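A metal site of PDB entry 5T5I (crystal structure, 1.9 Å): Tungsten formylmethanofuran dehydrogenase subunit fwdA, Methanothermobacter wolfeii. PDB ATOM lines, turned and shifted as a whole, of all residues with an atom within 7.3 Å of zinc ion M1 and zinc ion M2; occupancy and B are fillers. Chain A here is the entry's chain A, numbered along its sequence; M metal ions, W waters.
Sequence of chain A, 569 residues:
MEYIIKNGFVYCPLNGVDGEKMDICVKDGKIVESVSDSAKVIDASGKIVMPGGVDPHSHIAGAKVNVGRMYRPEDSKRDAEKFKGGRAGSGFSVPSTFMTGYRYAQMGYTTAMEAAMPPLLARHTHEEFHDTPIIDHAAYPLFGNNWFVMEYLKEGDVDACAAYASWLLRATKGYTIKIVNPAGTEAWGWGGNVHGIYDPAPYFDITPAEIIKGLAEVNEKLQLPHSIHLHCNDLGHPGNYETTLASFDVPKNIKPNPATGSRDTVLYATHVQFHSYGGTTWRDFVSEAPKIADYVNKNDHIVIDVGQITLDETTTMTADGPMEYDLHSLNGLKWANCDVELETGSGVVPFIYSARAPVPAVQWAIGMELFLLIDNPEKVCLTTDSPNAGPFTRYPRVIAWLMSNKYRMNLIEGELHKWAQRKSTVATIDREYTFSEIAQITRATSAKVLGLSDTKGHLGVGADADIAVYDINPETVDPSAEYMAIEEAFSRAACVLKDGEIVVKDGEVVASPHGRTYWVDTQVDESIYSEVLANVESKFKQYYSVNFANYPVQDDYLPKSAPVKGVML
Zinc ion M1 is bound by water W1, NE2 of His 59, NE2 of His 57, OD1 of Asp 385 and OQ1 of KCX 178.
Three residues have an atom within 4 Å of zinc ion M2: KCX 178, His 231 and His 271.
Zinc ion M2 is bound by water W1 (2.0 Å). OQ2 of KCX 178 is bound to zinc ion M2 (2.0 Å). Zinc ion M2 is bound by ND1 of His 231, at 2.1 Å. Zinc ion M2 is bound by NE2 of His 271, 2.2 Å away. Zinc ion M2 has four donor atoms within binding distance.
O of Asp 385 is in hydrogen-bond range of ND2 of Asn 388 (3.0 Å). The backbone carbonyl oxygen (O) of His 231 is in hydrogen-bond range of the backbone NH (N) of Asn 181 (3.0 Å). OG1 of Thr 270 sits at hydrogen-bond distance from ND1 of His 57 (3.0 Å). ND1 of His 57 sits at hydrogen-bond distance from NE2 of His 229, at 2.8 Å. The side-chain carboxylate (OD2) of Asp 320 sits at hydrogen-bond distance from a ring nitrogen (NE2) of His 231. The backbone NH (N) of His 231 is in hydrogen-bond range of the backbone carbonyl oxygen (O) of Ile 179, 2.8 Å away. The backbone carbonyl oxygen (O) of Ser 386 sits at hydrogen-bond distance from the backbone NH (N) of His 59, 2.9 Å away. NZ of KCX 178 is in hydrogen-bond range of O of Ala 115, at 3.0 Å.
Four residues have an atom within 4 Å of zinc ion M1: His 57, His 59, KCX 178 and Asp 385. The nearest printed residue that does not touch zinc ion M1 is His 271 (4.01 Å).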
ATOM      1  N   HIS A  57     -11.279   1.524  36.509  1.00  0.00           N
ATOM      2  CA  HIS A  57     -10.395   2.084  35.486  1.00  0.00           C
ATOM      3  C   HIS A  57      -8.980   2.301  36.005  1.00  0.00           C
ATOM      4  O   HIS A  57      -8.706   3.303  36.659  1.00  0.00           O
ATOM      5  CB  HIS A  57     -10.989   3.425  34.981  1.00  0.00           C
ATOM      6  CG  HIS A  57     -10.314   3.928  33.739  1.00  0.00           C
ATOM      7  ND1 HIS A  57     -10.968   3.891  32.525  1.00  0.00           N
ATOM      8  CD2 HIS A  57      -9.069   4.408  33.554  1.00  0.00           C
ATOM      9  CE1 HIS A  57     -10.130   4.394  31.653  1.00  0.00           C
ATOM     10  NE2 HIS A  57      -8.953   4.707  32.211  1.00  0.00           N
ATOM     11  N   SER A  58      -8.063   1.385  35.670  1.00  0.00           N
ATOM     12  CA  SER A  58      -6.664   1.492  36.059  1.00  0.00           C
ATOM     13  C   SER A  58      -5.762   0.913  34.957  1.00  0.00           C
ATOM     14  O   SER A  58      -6.218   0.056  34.184  1.00  0.00           O
ATOM     15  CB  SER A  58      -6.419   0.763  37.380  1.00  0.00           C
ATOM     16  OG  SER A  58      -5.235   1.217  38.000  1.00  0.00           O
ATOM     17  N   HIS A  59      -4.533   1.409  34.855  1.00  0.00           N
ATOM     18  CA  HIS A  59      -3.536   0.923  33.875  1.00  0.00           C
ATOM     19  C   HIS A  59      -2.541   0.112  34.682  1.00  0.00           C
ATOM     20  O   HIS A  59      -1.628   0.678  35.336  1.00  0.00           O
ATOM     21  CB  HIS A  59      -2.899   2.092  33.103  1.00  0.00           C
ATOM     22  CG  HIS A  59      -3.922   2.804  32.273  1.00  0.00           C
ATOM     23  ND1 HIS A  59      -4.257   2.368  31.008  1.00  0.00           N
ATOM     24  CD2 HIS A  59      -4.717   3.861  32.581  1.00  0.00           C
ATOM     25  CE1 HIS A  59      -5.191   3.181  30.566  1.00  0.00           C
ATOM     26  NE2 HIS A  59      -5.545   4.064  31.506  1.00  0.00           N
ATOM     27  N   ALA A 115      -7.702  -0.931  31.938  1.00  0.00           N
ATOM     28  CA  ALA A 115      -8.498   0.012  31.141  1.00  0.00           C
ATOM     29  C   ALA A 115      -8.230   0.058  29.646  1.00  0.00           C
ATOM     30  O   ALA A 115      -9.059   0.633  28.952  1.00  0.00           O
ATOM     31  CB  ALA A 115      -8.324   1.416  31.707  1.00  0.00           C
ATOM     32  N   ALA A 116      -7.110  -0.432  29.138  1.00  0.00           N
ATOM     33  CA  ALA A 116      -6.803  -0.238  27.711  1.00  0.00           C
ATOM     34  C   ALA A 116      -5.843  -1.311  27.191  1.00  0.00           C
ATOM     35  O   ALA A 116      -4.626  -1.146  27.275  1.00  0.00           O
ATOM     36  CB  ALA A 116      -6.178   1.146  27.523  1.00  0.00           C
ATOM     37  N   KCX A 178     -13.968  -0.480  24.829  1.00  0.00           N
ATOM     38  CA  KCX A 178     -13.255   0.741  25.238  1.00  0.00           C
ATOM     39  CB  KCX A 178     -11.952   0.342  25.934  1.00  0.00           C
ATOM     40  CG  KCX A 178     -11.111   1.545  26.369  1.00  0.00           C
ATOM     41  CD  KCX A 178     -11.709   2.281  27.567  1.00  0.00           C
ATOM     42  CE  KCX A 178     -11.027   3.618  27.805  1.00  0.00           C
ATOM     43  NZ  KCX A 178      -9.685   3.449  28.307  1.00  0.00           N
ATOM     44  C   KCX A 178     -12.984   1.594  24.024  1.00  0.00           C
ATOM     45  O   KCX A 178     -12.535   1.069  22.997  1.00  0.00           O
ATOM     46  CX  KCX A 178      -8.971   4.506  28.689  1.00  0.00           C
ATOM     47  OQ1 KCX A 178      -7.799   4.289  29.249  1.00  0.00           O
ATOM     48  OQ2 KCX A 178      -9.362   5.668  28.590  1.00  0.00           O
ATOM     49  N   ILE A 179     -13.283   2.908  24.129  1.00  0.00           N
ATOM     50  CA  ILE A 179     -13.134   3.891  23.057  1.00  0.00           C
ATOM     51  C   ILE A 179     -12.234   5.025  23.582  1.00  0.00           C
ATOM     52  O   ILE A 179     -12.632   5.744  24.507  1.00  0.00           O
ATOM     53  CB  ILE A 179     -14.504   4.419  22.599  1.00  0.00           C
ATOM     54  CG1 ILE A 179     -15.509   3.248  22.332  1.00  0.00           C
ATOM     55  CG2 ILE A 179     -14.352   5.321  21.376  1.00  0.00           C
ATOM     56  CD1 ILE A 179     -16.974   3.709  22.122  1.00  0.00           C
ATOM     57  N   VAL A 180     -11.066   5.216  22.941  1.00  0.00           N
ATOM     58  CA  VAL A 180     -10.074   6.256  23.289  1.00  0.00           C
ATOM     59  C   VAL A 180      -9.799   7.148  22.092  1.00  0.00           C
ATOM     60  O   VAL A 180      -9.228   6.671  21.095  1.00  0.00           O
ATOM     61  CB  VAL A 180      -8.744   5.635  23.808  1.00  0.00           C
ATOM     62  CG1 VAL A 180      -7.684   6.721  24.072  1.00  0.00           C
ATOM     63  CG2 VAL A 180      -8.979   4.784  25.051  1.00  0.00           C
ATOM     64  N   ASN A 181     -10.137   8.441  22.197  1.00  0.00           N
ATOM     65  CA  ASN A 181      -9.882   9.436  21.134  1.00  0.00           C
ATOM     66  C   ASN A 181     -10.323   8.858  19.770  1.00  0.00           C
ATOM     67  O   ASN A 181      -9.487   8.624  18.893  1.00  0.00           O
ATOM     68  CB  ASN A 181      -8.412   9.824  21.116  1.00  0.00           C
ATOM     69  CG  ASN A 181      -8.082  10.970  20.171  1.00  0.00           C
ATOM     70  OD1 ASN A 181      -8.941  11.750  19.773  1.00  0.00           O
ATOM     71  ND2 ASN A 181      -6.839  11.042  19.744  1.00  0.00           N
ATOM     72  N   HIS A 229     -17.241   2.472  27.107  1.00  0.00           N
ATOM     73  CA  HIS A 229     -16.394   3.151  28.109  1.00  0.00           C
ATOM     74  C   HIS A 229     -15.540   4.158  27.315  1.00  0.00           C
ATOM     75  O   HIS A 229     -14.699   3.748  26.535  1.00  0.00           O
ATOM     76  CB  HIS A 229     -15.605   2.055  28.832  1.00  0.00           C
ATOM     77  CG  HIS A 229     -14.940   2.453  30.110  1.00  0.00           C
ATOM     78  ND1 HIS A 229     -15.319   1.898  31.323  1.00  0.00           N
ATOM     79  CD2 HIS A 229     -13.873   3.259  30.327  1.00  0.00           C
ATOM     80  CE1 HIS A 229     -14.477   2.363  32.223  1.00  0.00           C
ATOM     81  NE2 HIS A 229     -13.590   3.200  31.686  1.00  0.00           N
ATOM     82  N   LEU A 230     -15.886   5.456  27.407  1.00  0.00           N
ATOM     83  CA  LEU A 230     -15.360   6.514  26.537  1.00  0.00           C
ATOM     84  C   LEU A 230     -14.401   7.513  27.156  1.00  0.00           C
ATOM     85  O   LEU A 230     -14.719   8.161  28.158  1.00  0.00           O
ATOM     86  CB  LEU A 230     -16.569   7.282  25.957  1.00  0.00           C
ATOM     87  CG  LEU A 230     -16.283   8.462  25.005  1.00  0.00           C
ATOM     88  CD1 LEU A 230     -15.563   8.005  23.715  1.00  0.00           C
ATOM     89  CD2 LEU A 230     -17.556   9.205  24.692  1.00  0.00           C
ATOM     90  N   HIS A 231     -13.242   7.673  26.496  1.00  0.00           N
ATOM     91  CA  HIS A 231     -12.212   8.691  26.726  1.00  0.00           C
ATOM     92  C   HIS A 231     -12.391   9.595  25.488  1.00  0.00           C
ATOM     93  O   HIS A 231     -12.090   9.191  24.356  1.00  0.00           O
ATOM     94  CB  HIS A 231     -10.822   8.014  26.846  1.00  0.00           C
ATOM     95  CG  HIS A 231      -9.576   8.848  26.583  1.00  0.00           C
ATOM     96  ND1 HIS A 231      -8.388   8.538  27.220  1.00  0.00           N
ATOM     97  CD2 HIS A 231      -9.314   9.787  25.641  1.00  0.00           C
ATOM     98  CE1 HIS A 231      -7.482   9.370  26.725  1.00  0.00           C
ATOM     99  NE2 HIS A 231      -7.996  10.128  25.767  1.00  0.00           N
ATOM    100  N   CYS A 232     -12.968  10.801  25.704  1.00  0.00           N
ATOM    101  CA  CYS A 232     -13.335  11.735  24.634  1.00  0.00           C
ATOM    102  C   CYS A 232     -12.187  12.237  23.789  1.00  0.00           C
ATOM    103  O   CYS A 232     -11.033  12.264  24.219  1.00  0.00           O
ATOM    104  CB  CYS A 232     -14.133  12.925  25.198  1.00  0.00           C
ATOM    105  SG  CYS A 232     -15.729  12.497  25.943  1.00  0.00           S
ATOM    106  N   LEU A 235      -8.760  15.662  24.581  1.00  0.00           N
ATOM    107  CA  LEU A 235      -8.335  15.594  25.975  1.00  0.00           C
ATOM    108  C   LEU A 235      -7.293  16.680  26.297  1.00  0.00           C
ATOM    109  O   LEU A 235      -6.364  16.904  25.531  1.00  0.00           O
ATOM    110  CB  LEU A 235      -7.728  14.223  26.327  1.00  0.00           C
ATOM    111  CG  LEU A 235      -7.475  13.932  27.840  1.00  0.00           C
ATOM    112  CD1 LEU A 235      -7.476  12.441  28.130  1.00  0.00           C
ATOM    113  CD2 LEU A 235      -6.101  14.435  28.344  1.00  0.00           C
ATOM    114  N   THR A 270     -15.017   8.263  31.204  1.00  0.00           N
ATOM    115  CA  THR A 270     -13.869   8.149  32.118  1.00  0.00           C
ATOM    116  C   THR A 270     -13.071   9.452  32.253  1.00  0.00           C
ATOM    117  O   THR A 270     -12.992  10.272  31.333  1.00  0.00           O
ATOM    118  CB  THR A 270     -12.990   6.928  31.725  1.00  0.00           C
ATOM    119  OG1 THR A 270     -12.016   6.717  32.758  1.00  0.00           O
ATOM    120  CG2 THR A 270     -12.321   7.084  30.346  1.00  0.00           C
ATOM    121  N   HIS A 271     -12.416   9.608  33.424  1.00  0.00           N
ATOM    122  CA  HIS A 271     -11.537  10.699  33.823  1.00  0.00           C
ATOM    123  C   HIS A 271     -11.979  12.055  33.259  1.00  0.00           C
ATOM    124  O   HIS A 271     -11.233  12.759  32.585  1.00  0.00           O
ATOM    125  CB  HIS A 271     -10.066  10.369  33.490  1.00  0.00           C
ATOM    126  CG  HIS A 271      -9.791   9.885  32.092  1.00  0.00           C
ATOM    127  ND1 HIS A 271      -9.955  10.692  30.986  1.00  0.00           N
ATOM    128  CD2 HIS A 271      -9.358   8.671  31.672  1.00  0.00           C
ATOM    129  CE1 HIS A 271      -9.616   9.945  29.940  1.00  0.00           C
ATOM    130  NE2 HIS A 271      -9.259   8.728  30.308  1.00  0.00           N
ATOM    131  N   PHE A 274     -10.191  15.776  32.992  1.00  0.00           N
ATOM    132  CA  PHE A 274      -9.385  16.190  31.828  1.00  0.00           C
ATOM    133  C   PHE A 274     -10.218  16.688  30.612  1.00  0.00           C
ATOM    134  O   PHE A 274      -9.638  17.124  29.620  1.00  0.00           O
ATOM    135  CB  PHE A 274      -8.482  15.035  31.341  1.00  0.00           C
ATOM    136  CG  PHE A 274      -7.400  14.569  32.279  1.00  0.00           C
ATOM    137  CD1 PHE A 274      -6.217  15.286  32.410  1.00  0.00           C
ATOM    138  CD2 PHE A 274      -7.513  13.353  32.933  1.00  0.00           C
ATOM    139  CE1 PHE A 274      -5.174  14.810  33.217  1.00  0.00           C
ATOM    140  CE2 PHE A 274      -6.456  12.871  33.723  1.00  0.00           C
ATOM    141  CZ  PHE A 274      -5.301  13.611  33.876  1.00  0.00           C
ATOM    142  N   HIS A 275     -11.556  16.576  30.687  1.00  0.00           N
ATOM    143  CA  HIS A 275     -12.516  16.923  29.663  1.00  0.00           C
ATOM    144  C   HIS A 275     -13.458  18.082  30.098  1.00  0.00           C
ATOM    145  O   HIS A 275     -14.433  18.350  29.405  1.00  0.00           O
ATOM    146  CB  HIS A 275     -13.319  15.648  29.361  1.00  0.00           C
ATOM    147  CG  HIS A 275     -12.472  14.555  28.808  1.00  0.00           C
ATOM    148  ND1 HIS A 275     -11.894  14.670  27.549  1.00  0.00           N
ATOM    149  CD2 HIS A 275     -12.058  13.403  29.378  1.00  0.00           C
ATOM    150  CE1 HIS A 275     -11.183  13.557  27.385  1.00  0.00           C
ATOM    151  NE2 HIS A 275     -11.276  12.763  28.446  1.00  0.00           N
ATOM    152  N   MET A 317       0.219   7.437  30.750  1.00  0.00           N
ATOM    153  CA  MET A 317       0.226   6.311  29.819  1.00  0.00           C
ATOM    154  C   MET A 317      -1.214   6.076  29.341  1.00  0.00           C
ATOM    155  O   MET A 317      -2.110   5.783  30.150  1.00  0.00           O
ATOM    156  CB  MET A 317       0.805   5.054  30.469  1.00  0.00           C
ATOM    157  CG  MET A 317       0.230   4.731  31.844  1.00  0.00           C
ATOM    158  SD  MET A 317       0.858   3.184  32.524  1.00  0.00           S
ATOM    159  CE  MET A 317       2.617   3.561  32.612  1.00  0.00           C
ATOM    160  N   THR A 318      -1.461   6.281  28.058  1.00  0.00           N
ATOM    161  CA  THR A 318      -2.803   6.133  27.514  1.00  0.00           C
ATOM    162  C   THR A 318      -2.727   5.575  26.113  1.00  0.00           C
ATOM    163  O   THR A 318      -1.644   5.568  25.523  1.00  0.00           O
ATOM    164  CB  THR A 318      -3.536   7.522  27.471  1.00  0.00           C
ATOM    165  OG1 THR A 318      -2.905   8.369  26.509  1.00  0.00           O
ATOM    166  CG2 THR A 318      -3.633   8.211  28.830  1.00  0.00           C
ATOM    167  N   ALA A 319      -3.882   5.192  25.548  1.00  0.00           N
ATOM    168  CA  ALA A 319      -3.970   4.797  24.139  1.00  0.00           C
ATOM    169  C   ALA A 319      -4.238   6.059  23.272  1.00  0.00           C
ATOM    170  O   ALA A 319      -4.691   5.925  22.135  1.00  0.00           O
ATOM    171  CB  ALA A 319      -5.081   3.762  23.934  1.00  0.00           C
ATOM    172  N   ASP A 320      -3.980   7.284  23.795  1.00  0.00           N
ATOM    173  CA  ASP A 320      -4.180   8.550  23.083  1.00  0.00           C
ATOM    174  C   ASP A 320      -2.782   9.016  22.658  1.00  0.00           C
ATOM    175  O   ASP A 320      -2.211   9.924  23.236  1.00  0.00           O
ATOM    176  CB  ASP A 320      -4.882   9.552  24.000  1.00  0.00           C
ATOM    177  CG  ASP A 320      -5.481  10.769  23.313  1.00  0.00           C
ATOM    178  OD1 ASP A 320      -5.026  11.101  22.171  1.00  0.00           O
ATOM    179  OD2 ASP A 320      -6.335  11.431  23.922  1.00  0.00           O
ATOM    180  N   MET A 323      -2.066  12.917  21.977  1.00  0.00           N
ATOM    181  CA  MET A 323      -2.071  13.693  23.211  1.00  0.00           C
ATOM    182  C   MET A 323      -0.724  13.509  23.960  1.00  0.00           C
ATOM    183  O   MET A 323      -0.167  14.469  24.479  1.00  0.00           O
ATOM    184  CB  MET A 323      -3.239  13.270  24.120  1.00  0.00           C
ATOM    185  CG  MET A 323      -3.307  14.036  25.433  1.00  0.00           C
ATOM    186  SD  MET A 323      -2.252  13.414  26.768  1.00  0.00           S
ATOM    187  CE  MET A 323      -3.056  11.873  27.154  1.00  0.00           C
ATOM    188  N   ASP A 385      -7.382   7.799  36.968  1.00  0.00           N
ATOM    189  CA  ASP A 385      -6.912   7.233  35.690  1.00  0.00           C
ATOM    190  C   ASP A 385      -5.516   6.635  35.921  1.00  0.00           C
ATOM    191  O   ASP A 385      -4.588   6.869  35.144  1.00  0.00           O
ATOM    192  CB  ASP A 385      -6.873   8.286  34.572  1.00  0.00           C
ATOM    193  CG  ASP A 385      -6.578   7.699  33.186  1.00  0.00           C
ATOM    194  OD1 ASP A 385      -6.816   6.483  32.997  1.00  0.00           O
ATOM    195  OD2 ASP A 385      -6.136   8.456  32.291  1.00  0.00           O
ATOM    196  N   SER A 386      -5.352   5.933  37.048  1.00  0.00           N
ATOM    197  CA  SER A 386      -4.047   5.501  37.540  1.00  0.00           C
ATOM    198  C   SER A 386      -3.147   4.928  36.483  1.00  0.00           C
ATOM    199  O   SER A 386      -3.596   4.057  35.734  1.00  0.00           O
ATOM    200  CB  SER A 386      -4.180   4.519  38.698  1.00  0.00           C
ATOM    201  OG  SER A 386      -2.908   4.229  39.254  1.00  0.00           O
ATOM    202  N   ASN A 388      -2.088   8.114  35.498  1.00  0.00           N
ATOM    203  CA  ASN A 388      -2.158   9.392  34.773  1.00  0.00           C
ATOM    204  C   ASN A 388      -2.413  10.644  35.607  1.00  0.00           C
ATOM    205  O   ASN A 388      -1.696  11.628  35.403  1.00  0.00           O
ATOM    206  CB  ASN A 388      -3.166   9.340  33.652  1.00  0.00           C
ATOM    207  CG  ASN A 388      -2.738   8.488  32.517  1.00  0.00           C
ATOM    208  OD1 ASN A 388      -2.028   8.955  31.635  1.00  0.00           O
ATOM    209  ND2 ASN A 388      -3.176   7.238  32.496  1.00  0.00           N
HETATM  210 ZN    ZN M   1      -7.183   5.338  31.224  1.00  0.00          ZN
HETATM  211 ZN    ZN M   2      -8.260   7.338  28.985  1.00  0.00          ZN
HETATM  212  O   HOH W   1      -6.679   6.927  30.093  1.00  0.00           O
HETATM  213  O   HOH W   2      -5.941   5.349  27.654  1.00  0.00           O
